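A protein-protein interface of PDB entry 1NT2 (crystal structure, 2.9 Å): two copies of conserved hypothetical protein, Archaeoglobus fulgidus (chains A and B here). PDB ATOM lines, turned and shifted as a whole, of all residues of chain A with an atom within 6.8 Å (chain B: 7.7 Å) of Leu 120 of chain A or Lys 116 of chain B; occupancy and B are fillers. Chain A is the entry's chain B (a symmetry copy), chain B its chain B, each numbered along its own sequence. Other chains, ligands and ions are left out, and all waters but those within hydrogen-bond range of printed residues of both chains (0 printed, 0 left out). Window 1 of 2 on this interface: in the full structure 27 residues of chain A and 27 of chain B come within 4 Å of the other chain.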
ATOM      1  N   ILE A  87      11.110   4.883  -2.692  1.00  0.00           N
ATOM      2  CA  ILE A  87      12.257   4.791  -3.573  1.00  0.00           C
ATOM      3  C   ILE A  87      12.010   5.697  -4.758  1.00  0.00           C
ATOM      4  O   ILE A  87      12.942   6.228  -5.351  1.00  0.00           O
ATOM      5  CB  ILE A  87      12.413   3.365  -4.087  1.00  0.00           C
ATOM      6  CG1 ILE A  87      12.600   2.424  -2.906  1.00  0.00           C
ATOM      7  CG2 ILE A  87      13.579   3.278  -5.040  1.00  0.00           C
ATOM      8  CD1 ILE A  87      12.460   0.987  -3.270  1.00  0.00           C
ATOM      9  N   SER A  90      12.310   9.742  -3.867  1.00  0.00           N
ATOM     10  CA  SER A  90      13.698  10.192  -3.915  1.00  0.00           C
ATOM     11  C   SER A  90      14.195  10.333  -5.342  1.00  0.00           C
ATOM     12  O   SER A  90      14.830  11.326  -5.687  1.00  0.00           O
ATOM     13  CB  SER A  90      14.589   9.202  -3.182  1.00  0.00           C
ATOM     14  OG  SER A  90      13.976   8.805  -1.975  1.00  0.00           O
ATOM     15  N   ILE A  91      13.923   9.333  -6.171  1.00  0.00           N
ATOM     16  CA  ILE A  91      14.356   9.394  -7.554  1.00  0.00           C
ATOM     17  C   ILE A  91      14.067  10.787  -8.084  1.00  0.00           C
ATOM     18  O   ILE A  91      14.871  11.334  -8.822  1.00  0.00           O
ATOM     19  CB  ILE A  91      13.599   8.387  -8.444  1.00  0.00           C
ATOM     20  CG1 ILE A  91      14.056   6.955  -8.161  1.00  0.00           C
ATOM     21  CG2 ILE A  91      13.823   8.727  -9.900  1.00  0.00           C
ATOM     22  CD1 ILE A  91      15.457   6.667  -8.612  1.00  0.00           C
ATOM     23  N   LEU A  94      15.669  14.094  -6.247  1.00  0.00           N
ATOM     24  CA  LEU A  94      17.107  13.931  -6.369  1.00  0.00           C
ATOM     25  C   LEU A  94      17.463  14.287  -7.801  1.00  0.00           C
ATOM     26  O   LEU A  94      18.625  14.316  -8.180  1.00  0.00           O
ATOM     27  CB  LEU A  94      17.501  12.496  -6.084  1.00  0.00           C
ATOM     28  CG  LEU A  94      18.386  12.301  -4.867  1.00  0.00           C
ATOM     29  CD1 LEU A  94      17.727  12.859  -3.613  1.00  0.00           C
ATOM     30  CD2 LEU A  94      18.647  10.829  -4.724  1.00  0.00           C
ATOM     31  N   GLU A 114      24.133  11.248 -11.585  1.00  0.00           N
ATOM     32  CA  GLU A 114      23.383  10.560 -12.623  1.00  0.00           C
ATOM     33  C   GLU A 114      23.430   9.046 -12.517  1.00  0.00           C
ATOM     34  O   GLU A 114      22.394   8.389 -12.530  1.00  0.00           O
ATOM     35  CB  GLU A 114      23.883  10.974 -14.000  1.00  0.00           C
ATOM     36  CG  GLU A 114      23.403  12.332 -14.433  1.00  0.00           C
ATOM     37  CD  GLU A 114      23.822  12.644 -15.849  1.00  0.00           C
ATOM     38  OE1 GLU A 114      23.473  11.858 -16.759  1.00  0.00           O
ATOM     39  OE2 GLU A 114      24.503  13.672 -16.053  1.00  0.00           O
ATOM     40  N   LYS A 115      24.623   8.482 -12.425  1.00  0.00           N
ATOM     41  CA  LYS A 115      24.726   7.041 -12.316  1.00  0.00           C
ATOM     42  C   LYS A 115      24.018   6.521 -11.063  1.00  0.00           C
ATOM     43  O   LYS A 115      23.326   5.508 -11.121  1.00  0.00           O
ATOM     44  CB  LYS A 115      26.195   6.609 -12.324  1.00  0.00           C
ATOM     45  CG  LYS A 115      26.846   6.637 -13.717  1.00  0.00           C
ATOM     46  CD  LYS A 115      27.130   8.055 -14.234  1.00  0.00           C
ATOM     47  CE  LYS A 115      28.530   8.529 -13.847  1.00  0.00           C
ATOM     48  NZ  LYS A 115      29.599   7.725 -14.511  1.00  0.00           N
ATOM     49  N   LYS A 116      24.169   7.220  -9.938  1.00  0.00           N
ATOM     50  CA  LYS A 116      23.537   6.809  -8.680  1.00  0.00           C
ATOM     51  C   LYS A 116      22.015   6.908  -8.782  1.00  0.00           C
ATOM     52  O   LYS A 116      21.298   6.110  -8.193  1.00  0.00           O
ATOM     53  CB  LYS A 116      24.056   7.676  -7.529  1.00  0.00           C
ATOM     54  CG  LYS A 116      23.983   7.040  -6.140  1.00  0.00           C
ATOM     55  CD  LYS A 116      24.702   5.686  -6.075  1.00  0.00           C
ATOM     56  CE  LYS A 116      26.157   5.745  -6.562  1.00  0.00           C
ATOM     57  NZ  LYS A 116      27.066   6.413  -5.604  1.00  0.00           N
ATOM     58  N   ILE A 117      21.520   7.894  -9.526  1.00  0.00           N
ATOM     59  CA  ILE A 117      20.081   8.036  -9.713  1.00  0.00           C
ATOM     60  C   ILE A 117      19.681   6.782 -10.462  1.00  0.00           C
ATOM     61  O   ILE A 117      18.833   6.029 -10.004  1.00  0.00           O
ATOM     62  CB  ILE A 117      19.720   9.273 -10.567  1.00  0.00           C
ATOM     63  CG1 ILE A 117      19.920  10.551  -9.753  1.00  0.00           C
ATOM     64  CG2 ILE A 117      18.283   9.194 -11.029  1.00  0.00           C
ATOM     65  CD1 ILE A 117      19.002  10.683  -8.573  1.00  0.00           C
ATOM     66  N   ARG A 118      20.327   6.560 -11.606  1.00  0.00           N
ATOM     67  CA  ARG A 118      20.091   5.394 -12.458  1.00  0.00           C
ATOM     68  C   ARG A 118      20.118   4.100 -11.630  1.00  0.00           C
ATOM     69  O   ARG A 118      19.182   3.305 -11.669  1.00  0.00           O
ATOM     70  CB  ARG A 118      21.170   5.344 -13.551  1.00  0.00           C
ATOM     71  CG  ARG A 118      20.683   5.031 -14.974  1.00  0.00           C
ATOM     72  CD  ARG A 118      21.400   5.926 -16.005  1.00  0.00           C
ATOM     73  NE  ARG A 118      22.863   5.853 -15.888  1.00  0.00           N
ATOM     74  CZ  ARG A 118      23.714   6.809 -16.281  1.00  0.00           C
ATOM     75  NH1 ARG A 118      23.262   7.938 -16.829  1.00  0.00           N
ATOM     76  NH2 ARG A 118      25.025   6.639 -16.114  1.00  0.00           N
ATOM     77  N   GLU A 119      21.196   3.902 -10.878  1.00  0.00           N
ATOM     78  CA  GLU A 119      21.347   2.711 -10.043  1.00  0.00           C
ATOM     79  C   GLU A 119      20.149   2.564  -9.115  1.00  0.00           C
ATOM     80  O   GLU A 119      19.775   1.458  -8.725  1.00  0.00           O
ATOM     81  CB  GLU A 119      22.620   2.812  -9.192  1.00  0.00           C
ATOM     82  CG  GLU A 119      23.921   2.986  -9.978  1.00  0.00           C
ATOM     83  CD  GLU A 119      25.141   3.120  -9.068  1.00  0.00           C
ATOM     84  OE1 GLU A 119      25.483   2.133  -8.384  1.00  0.00           O
ATOM     85  OE2 GLU A 119      25.759   4.209  -9.027  1.00  0.00           O
ATOM     86  N   LEU A 120      19.563   3.705  -8.773  1.00  0.00           N
ATOM     87  CA  LEU A 120      18.416   3.789  -7.875  1.00  0.00           C
ATOM     88  C   LEU A 120      17.098   3.561  -8.629  1.00  0.00           C
ATOM     89  O   LEU A 120      16.157   2.985  -8.082  1.00  0.00           O
ATOM     90  CB  LEU A 120      18.422   5.171  -7.203  1.00  0.00           C
ATOM     91  CG  LEU A 120      17.644   5.474  -5.920  1.00  0.00           C
ATOM     92  CD1 LEU A 120      18.183   4.649  -4.760  1.00  0.00           C
ATOM     93  CD2 LEU A 120      17.777   6.969  -5.623  1.00  0.00           C
ATOM     94  N   ARG A 121      17.041   4.024  -9.879  1.00  0.00           N
ATOM     95  CA  ARG A 121      15.856   3.879 -10.733  1.00  0.00           C
ATOM     96  C   ARG A 121      15.816   2.410 -11.168  1.00  0.00           C
ATOM     97  O   ARG A 121      14.871   1.941 -11.803  1.00  0.00           O
ATOM     98  CB  ARG A 121      15.979   4.819 -11.950  1.00  0.00           C
ATOM     99  CG  ARG A 121      14.656   5.377 -12.497  1.00  0.00           C
ATOM    100  CD  ARG A 121      14.837   6.778 -13.101  1.00  0.00           C
ATOM    101  NE  ARG A 121      15.656   6.775 -14.314  1.00  0.00           N
ATOM    102  CZ  ARG A 121      16.183   7.863 -14.877  1.00  0.00           C
ATOM    103  NH1 ARG A 121      15.986   9.062 -14.338  1.00  0.00           N
ATOM    104  NH2 ARG A 121      16.902   7.751 -15.990  1.00  0.00           N
ATOM    105  N   GLU A 122      16.871   1.696 -10.792  1.00  0.00           N
ATOM    106  CA  GLU A 122      17.022   0.283 -11.083  1.00  0.00           C
ATOM    107  C   GLU A 122      16.375  -0.507  -9.958  1.00  0.00           C
ATOM    108  O   GLU A 122      15.598  -1.421 -10.202  1.00  0.00           O
ATOM    109  CB  GLU A 122      18.507  -0.063 -11.170  1.00  0.00           C
ATOM    110  CG  GLU A 122      18.804  -1.550 -11.199  1.00  0.00           C
ATOM    111  CD  GLU A 122      20.293  -1.832 -11.131  1.00  0.00           C
ATOM    112  OE1 GLU A 122      21.019  -1.385 -12.050  1.00  0.00           O
ATOM    113  OE2 GLU A 122      20.730  -2.494 -10.159  1.00  0.00           O
ATOM    114  N   LEU A 123      16.707  -0.146  -8.722  1.00  0.00           N
ATOM    115  CA  LEU A 123      16.151  -0.808  -7.548  1.00  0.00           C
ATOM    116  C   LEU A 123      14.640  -0.679  -7.608  1.00  0.00           C
ATOM    117  O   LEU A 123      13.919  -1.569  -7.173  1.00  0.00           O
ATOM    118  CB  LEU A 123      16.663  -0.148  -6.269  1.00  0.00           C
ATOM    119  CG  LEU A 123      16.294  -0.811  -4.945  1.00  0.00           C
ATOM    120  CD1 LEU A 123      17.111  -2.063  -4.796  1.00  0.00           C
ATOM    121  CD2 LEU A 123      16.583   0.116  -3.786  1.00  0.00           C
ATOM    122  N   ARG A 124      14.166   0.443  -8.141  1.00  0.00           N
ATOM    123  CA  ARG A 124      12.740   0.667  -8.267  1.00  0.00           C
ATOM    124  C   ARG A 124      12.153  -0.382  -9.198  1.00  0.00           C
ATOM    125  O   ARG A 124      11.171  -1.037  -8.862  1.00  0.00           O
ATOM    126  CB  ARG A 124      12.451   2.059  -8.829  1.00  0.00           C
ATOM    127  CG  ARG A 124      10.996   2.248  -9.252  1.00  0.00           C
ATOM    128  CD  ARG A 124      10.792   3.528 -10.040  1.00  0.00           C
ATOM    129  NE  ARG A 124       9.669   3.424 -10.978  1.00  0.00           N
ATOM    130  CZ  ARG A 124       9.671   2.684 -12.090  1.00  0.00           C
ATOM    131  NH1 ARG A 124      10.743   1.972 -12.415  1.00  0.00           N
ATOM    132  NH2 ARG A 124       8.602   2.655 -12.883  1.00  0.00           N
ATOM    133  N   ARG A 125      12.752  -0.533 -10.375  1.00  0.00           N
ATOM    134  CA  ARG A 125      12.282  -1.517 -11.350  1.00  0.00           C
ATOM    135  C   ARG A 125      12.559  -2.926 -10.820  1.00  0.00           C
ATOM    136  O   ARG A 125      12.107  -3.907 -11.400  1.00  0.00           O
ATOM    137  CB  ARG A 125      12.991  -1.326 -12.697  1.00  0.00           C
ATOM    138  CG  ARG A 125      12.767   0.028 -13.363  1.00  0.00           C
ATOM    139  CD  ARG A 125      11.707  -0.028 -14.462  1.00  0.00           C
ATOM    140  NE  ARG A 125      10.352  -0.260 -13.956  1.00  0.00           N
ATOM    141  CZ  ARG A 125       9.264  -0.360 -14.727  1.00  0.00           C
ATOM    142  NH1 ARG A 125       9.358  -0.251 -16.049  1.00  0.00           N
ATOM    143  NH2 ARG A 125       8.072  -0.567 -14.177  1.00  0.00           N
ATOM    144  N   ASP A 126      13.308  -3.009  -9.723  1.00  0.00           N
ATOM    145  CA  ASP A 126      13.647  -4.281  -9.089  1.00  0.00           C
ATOM    146  C   ASP A 126      12.549  -4.658  -8.103  1.00  0.00           C
ATOM    147  O   ASP A 126      12.123  -5.811  -8.038  1.00  0.00           O
ATOM    148  CB  ASP A 126      14.977  -4.156  -8.343  1.00  0.00           C
ATOM    149  CG  ASP A 126      16.145  -4.755  -9.108  1.00  0.00           C
ATOM    150  OD1 ASP A 126      16.219  -4.592 -10.348  1.00  0.00           O
ATOM    151  OD2 ASP A 126      17.002  -5.380  -8.450  1.00  0.00           O
ATOM    152  N   SER B  90      16.856  10.891   2.121  1.00  0.00           N
ATOM    153  CA  SER B  90      16.510   9.598   1.541  1.00  0.00           C
ATOM    154  C   SER B  90      17.243   8.458   2.226  1.00  0.00           C
ATOM    155  O   SER B  90      16.645   7.436   2.548  1.00  0.00           O
ATOM    156  CB  SER B  90      16.856   9.583   0.061  1.00  0.00           C
ATOM    157  OG  SER B  90      16.461  10.798  -0.537  1.00  0.00           O
ATOM    158  N   ILE B  91      18.543   8.625   2.434  1.00  0.00           N
ATOM    159  CA  ILE B  91      19.314   7.586   3.090  1.00  0.00           C
ATOM    160  C   ILE B  91      18.516   7.075   4.276  1.00  0.00           C
ATOM    161  O   ILE B  91      18.509   5.882   4.533  1.00  0.00           O
ATOM    162  CB  ILE B  91      20.661   8.115   3.624  1.00  0.00           C
ATOM    163  CG1 ILE B  91      21.637   8.385   2.476  1.00  0.00           C
ATOM    164  CG2 ILE B  91      21.256   7.111   4.586  1.00  0.00           C
ATOM    165  CD1 ILE B  91      22.122   7.143   1.789  1.00  0.00           C
ATOM    166  N   LEU B  94      14.749   5.524   3.746  1.00  0.00           N
ATOM    167  CA  LEU B  94      14.937   4.368   2.886  1.00  0.00           C
ATOM    168  C   LEU B  94      15.503   3.265   3.762  1.00  0.00           C
ATOM    169  O   LEU B  94      15.693   2.139   3.325  1.00  0.00           O
ATOM    170  CB  LEU B  94      15.914   4.692   1.774  1.00  0.00           C
ATOM    171  CG  LEU B  94      15.334   4.639   0.373  1.00  0.00           C
ATOM    172  CD1 LEU B  94      14.146   5.580   0.234  1.00  0.00           C
ATOM    173  CD2 LEU B  94      16.426   5.013  -0.587  1.00  0.00           C
ATOM    174  N   THR B 110      16.001  -7.483  -0.222  1.00  0.00           N
ATOM    175  CA  THR B 110      16.275  -6.561   0.870  1.00  0.00           C
ATOM    176  C   THR B 110      17.779  -6.323   0.841  1.00  0.00           C
ATOM    177  O   THR B 110      18.276  -5.315   1.342  1.00  0.00           O
ATOM    178  CB  THR B 110      15.887  -7.162   2.239  1.00  0.00           C
ATOM    179  OG1 THR B 110      16.564  -8.407   2.425  1.00  0.00           O
ATOM    180  CG2 THR B 110      14.395  -7.393   2.322  1.00  0.00           C
ATOM    181  N   GLU B 111      18.496  -7.266   0.239  1.00  0.00           N
ATOM    182  CA  GLU B 111      19.942  -7.164   0.131  1.00  0.00           C
ATOM    183  C   GLU B 111      20.318  -6.142  -0.920  1.00  0.00           C
ATOM    184  O   GLU B 111      21.189  -5.302  -0.683  1.00  0.00           O
ATOM    185  CB  GLU B 111      20.555  -8.520  -0.222  1.00  0.00           C
ATOM    186  CG  GLU B 111      20.478  -9.540   0.904  1.00  0.00           C
ATOM    187  CD  GLU B 111      21.006  -8.998   2.231  1.00  0.00           C
ATOM    188  OE1 GLU B 111      22.182  -8.559   2.284  1.00  0.00           O
ATOM    189  OE2 GLU B 111      20.235  -9.012   3.222  1.00  0.00           O
ATOM    190  N   LYS B 112      19.668  -6.216  -2.081  1.00  0.00           N
ATOM    191  CA  LYS B 112      19.943  -5.263  -3.154  1.00  0.00           C
ATOM    192  C   LYS B 112      19.685  -3.868  -2.617  1.00  0.00           C
ATOM    193  O   LYS B 112      20.268  -2.886  -3.072  1.00  0.00           O
ATOM    194  CB  LYS B 112      19.048  -5.520  -4.376  1.00  0.00           C
ATOM    195  CG  LYS B 112      19.435  -6.755  -5.183  1.00  0.00           C
ATOM    196  CD  LYS B 112      18.696  -6.818  -6.512  1.00  0.00           C
ATOM    197  CE  LYS B 112      19.030  -8.104  -7.257  1.00  0.00           C
ATOM    198  NZ  LYS B 112      18.341  -8.210  -8.572  1.00  0.00           N
ATOM    199  N   PHE B 113      18.802  -3.802  -1.631  1.00  0.00           N
ATOM    200  CA  PHE B 113      18.452  -2.547  -0.994  1.00  0.00           C
ATOM    201  C   PHE B 113      19.698  -2.076  -0.255  1.00  0.00           C
ATOM    202  O   PHE B 113      20.270  -1.043  -0.583  1.00  0.00           O
ATOM    203  CB  PHE B 113      17.288  -2.776  -0.020  1.00  0.00           C
ATOM    204  CG  PHE B 113      16.263  -1.679  -0.024  1.00  0.00           C
ATOM    205  CD1 PHE B 113      16.309  -0.659   0.915  1.00  0.00           C
ATOM    206  CD2 PHE B 113      15.256  -1.659  -0.971  1.00  0.00           C
ATOM    207  CE1 PHE B 113      15.361   0.368   0.908  1.00  0.00           C
ATOM    208  CE2 PHE B 113      14.308  -0.637  -0.983  1.00  0.00           C
ATOM    209  CZ  PHE B 113      14.362   0.375  -0.042  1.00  0.00           C
ATOM    210  N   GLU B 114      20.126  -2.856   0.730  1.00  0.00           N
ATOM    211  CA  GLU B 114      21.306  -2.517   1.509  1.00  0.00           C
ATOM    212  C   GLU B 114      22.456  -1.974   0.679  1.00  0.00           C
ATOM    213  O   GLU B 114      23.002  -0.920   0.988  1.00  0.00           O
ATOM    214  CB  GLU B 114      21.790  -3.729   2.291  1.00  0.00           C
ATOM    215  CG  GLU B 114      20.965  -4.028   3.513  1.00  0.00           C
ATOM    216  CD  GLU B 114      21.555  -5.159   4.319  1.00  0.00           C
ATOM    217  OE1 GLU B 114      22.733  -5.045   4.729  1.00  0.00           O
ATOM    218  OE2 GLU B 114      20.845  -6.163   4.541  1.00  0.00           O
ATOM    219  N   LYS B 115      22.841  -2.690  -0.364  1.00  0.00           N
ATOM    220  CA  LYS B 115      23.931  -2.216  -1.193  1.00  0.00           C
ATOM    221  C   LYS B 115      23.607  -0.860  -1.824  1.00  0.00           C
ATOM    222  O   LYS B 115      24.462   0.021  -1.864  1.00  0.00           O
ATOM    223  CB  LYS B 115      24.266  -3.247  -2.275  1.00  0.00           C
ATOM    224  CG  LYS B 115      25.068  -4.454  -1.759  1.00  0.00           C
ATOM    225  CD  LYS B 115      24.236  -5.427  -0.911  1.00  0.00           C
ATOM    226  CE  LYS B 115      23.609  -6.529  -1.764  1.00  0.00           C
ATOM    227  NZ  LYS B 115      24.639  -7.427  -2.367  1.00  0.00           N
ATOM    228  N   LYS B 116      22.374  -0.680  -2.296  1.00  0.00           N
ATOM    229  CA  LYS B 116      21.960   0.579  -2.922  1.00  0.00           C
ATOM    230  C   LYS B 116      21.958   1.716  -1.900  1.00  0.00           C
ATOM    231  O   LYS B 116      22.254   2.856  -2.236  1.00  0.00           O
ATOM    232  CB  LYS B 116      20.571   0.417  -3.549  1.00  0.00           C
ATOM    233  CG  LYS B 116      20.254   1.370  -4.701  1.00  0.00           C
ATOM    234  CD  LYS B 116      21.293   1.299  -5.828  1.00  0.00           C
ATOM    235  CE  LYS B 116      21.520  -0.125  -6.356  1.00  0.00           C
ATOM    236  NZ  LYS B 116      20.402  -0.624  -7.188  1.00  0.00           N
ATOM    237  N   ILE B 117      21.616   1.409  -0.652  1.00  0.00           N
ATOM    238  CA  ILE B 117      21.630   2.423   0.396  1.00  0.00           C
ATOM    239  C   ILE B 117      23.088   2.819   0.506  1.00  0.00           C
ATOM    240  O   ILE B 117      23.427   3.984   0.355  1.00  0.00           O
ATOM    241  CB  ILE B 117      21.151   1.866   1.757  1.00  0.00           C
ATOM    242  CG1 ILE B 117      19.638   1.654   1.735  1.00  0.00           C
ATOM    243  CG2 ILE B 117      21.506   2.824   2.872  1.00  0.00           C
ATOM    244  CD1 ILE B 117      18.838   2.915   1.592  1.00  0.00           C
ATOM    245  N   ARG B 118      23.941   1.825   0.745  1.00  0.00           N
ATOM    246  CA  ARG B 118      25.388   2.009   0.867  1.00  0.00           C
ATOM    247  C   ARG B 118      25.931   2.840  -0.305  1.00  0.00           C
ATOM    248  O   ARG B 118      26.603   3.850  -0.107  1.00  0.00           O
ATOM    249  CB  ARG B 118      26.068   0.632   0.897  1.00  0.00           C
ATOM    250  CG  ARG B 118      27.174   0.443   1.947  1.00  0.00           C
ATOM    251  CD  ARG B 118      27.064  -0.945   2.612  1.00  0.00           C
ATOM    252  NE  ARG B 118      27.037  -2.036   1.629  1.00  0.00           N
ATOM    253  CZ  ARG B 118      26.495  -3.242   1.835  1.00  0.00           C
ATOM    254  NH1 ARG B 118      25.922  -3.540   3.001  1.00  0.00           N
ATOM    255  NH2 ARG B 118      26.517  -4.154   0.863  1.00  0.00           N
ATOM    256  N   GLU B 119      25.630   2.408  -1.526  1.00  0.00           N
ATOM    257  CA  GLU B 119      26.084   3.108  -2.727  1.00  0.00           C
ATOM    258  C   GLU B 119      25.662   4.569  -2.677  1.00  0.00           C
ATOM    259  O   GLU B 119      26.320   5.445  -3.238  1.00  0.00           O
ATOM    260  CB  GLU B 119      25.481   2.463  -3.982  1.00  0.00           C
ATOM    261  CG  GLU B 119      25.797   0.978  -4.171  1.00  0.00           C
ATOM    262  CD  GLU B 119      25.133   0.394  -5.417  1.00  0.00           C
ATOM    263  OE1 GLU B 119      25.513   0.795  -6.537  1.00  0.00           O
ATOM    264  OE2 GLU B 119      24.228  -0.463  -5.285  1.00  0.00           O
ATOM    265  N   LEU B 120      24.549   4.807  -1.993  1.00  0.00           N
ATOM    266  CA  LEU B 120      23.958   6.132  -1.842  1.00  0.00           C
ATOM    267  C   LEU B 120      24.605   6.904  -0.683  1.00  0.00           C
ATOM    268  O   LEU B 120      24.751   8.125  -0.750  1.00  0.00           O
ATOM    269  CB  LEU B 120      22.448   5.970  -1.607  1.00  0.00           C
ATOM    270  CG  LEU B 120      21.447   7.109  -1.817  1.00  0.00           C
ATOM    271  CD1 LEU B 120      21.411   7.527  -3.279  1.00  0.00           C
ATOM    272  CD2 LEU B 120      20.070   6.624  -1.362  1.00  0.00           C
ATOM    273  N   ARG B 121      24.981   6.183   0.374  1.00  0.00           N
ATOM    274  CA  ARG B 121      25.620   6.770   1.558  1.00  0.00           C
ATOM    275  C   ARG B 121      27.058   7.105   1.149  1.00  0.00           C
ATOM    276  O   ARG B 121      27.824   7.719   1.892  1.00  0.00           O
ATOM    277  CB  ARG B 121      25.590   5.754   2.718  1.00  0.00           C
ATOM    278  CG  ARG B 121      25.484   6.356   4.128  1.00  0.00           C
ATOM    279  CD  ARG B 121      24.718   5.429   5.085  1.00  0.00           C
ATOM    280  NE  ARG B 121      25.436   4.186   5.370  1.00  0.00           N
ATOM    281  CZ  ARG B 121      24.894   3.110   5.942  1.00  0.00           C
ATOM    282  NH1 ARG B 121      23.612   3.110   6.296  1.00  0.00           N
ATOM    283  NH2 ARG B 121      25.640   2.033   6.171  1.00  0.00           N
ATOM    284  N   GLU B 122      27.395   6.691  -0.067  1.00  0.00           N
ATOM    285  CA  GLU B 122      28.700   6.922  -0.656  1.00  0.00           C
ATOM    286  C   GLU B 122      28.669   8.262  -1.372  1.00  0.00           C
ATOM    287  O   GLU B 122      29.557   9.086  -1.194  1.00  0.00           O
ATOM    288  CB  GLU B 122      29.013   5.809  -1.654  1.00  0.00           C
ATOM    289  CG  GLU B 122      30.221   6.076  -2.532  1.00  0.00           C
ATOM    290  CD  GLU B 122      30.390   5.014  -3.601  1.00  0.00           C
ATOM    291  OE1 GLU B 122      30.572   3.830  -3.231  1.00  0.00           O
ATOM    292  OE2 GLU B 122      30.336   5.364  -4.805  1.00  0.00           O
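Ser 90 of chain A touches Leu 94 of chain B, and with the chains exchanged Leu 94 of chain A touches Ser 90 of chain B. Lys 116 of chain A touches Leu 120 of chain B, and with the chains exchanged Leu 120 of chain A touches Lys 116 of chain B. Lys 116 of chain A touches Glu 122 of chain B, and with the chains exchanged Glu 122 of chain A touches Lys 116 of chain B. Glu 119 of chain A touches its own counterpart, Glu 119 of chain B. Positions printed for both chains: 90, 91, 94, 114, 115, 116, 117, 118, 119, 120, 121 and 122. Of the 15 pairs that touch across the chains among the printed residues, 10 have their exchanged pair printed and touching as well.
Ile 87 of chain A touches Phe 113 of chain B. Leu 94 of chain B touches Ser 90 of chain A (CD1 to OG, 3.9 Å). OG of Ser 90 of chain B touches CD1 of Leu 94 of chain A, 3.9 Å away. CG of Lys 116 of chain A touches CD1 of Leu 120 of chain B, 3.9 Å away. Leu 120 of chain A touches Lys 116 of chain B (CD1 to CG, 3.9 Å). Leu 123 of chain A touches Lys 112 of chain B (CD1 to O, 3.7 Å). Phe 113 of chain B touches Leu 123 of chain A (CD2 to CD2, 3.6 Å). Lys 116 of chain B touches Leu 123 of chain A.
Printed residues of chain A that touch a printed residue of chain B: Ile 87, Ser 90, Leu 94, Lys 116, Glu 119, Leu 120, Glu 122, Leu 123 and Asp 126. Among the printed residues, 15 pairs touch across the chains.
The side-chain hydroxyl of Ser 90 of chain B sits at hydrogen-bond distance from the side-chain hydroxyl of Ser 90 of chain A, 3.5 Å away. OD2 of Asp 126 of chain A lies within salt-bridge range of NZ of Lys 112 of chain B, at 3.1 Å. The backbone carbonyl oxygen (O) of Glu 119 of chain A sits at hydrogen-bond distance from the side-chain amino group (NZ) of Lys 116 of chain B (2.7 Å). OE2 of Glu 122 of chain A is in salt-bridge range of NZ of Lys 116 of chain B (3.5 Å). O of Glu 119 of chain B is in hydrogen-bond range of NZ of Lys 116 of chain A (2.7 Å). The side-chain amino group (NZ) of Lys 116 of chain A lies within salt-bridge range of the side-chain carboxylate (OE2) of Glu 122 of chain B (3.5 Å). The side-chain carboxylate (OE1) of Glu 119 of chain A sits close to the side-chain carboxylate (OE1) of Glu 119 of chain B, 2.3 Å away.
Of the printed residues of chain B, Ser 90 of chain A touches Ser 90 and Leu 94. Printed residues of chain B within 4 Å of Leu 94 of chain A: Ser 90. Ile 117 of chain A touches none of the printed residues of chain B. Of the printed residues of chain B, Leu 120 of chain A touches Lys 116. Of the printed residues of chain A, Leu 94 of chain B touches Ser 90. Of the printed residues of chain A, Lys 112 of chain B touches Leu 123 (3.7 Å) and Asp 126 (2.9 Å). Arg 121 of chain B touches none of the printed residues of chain A.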
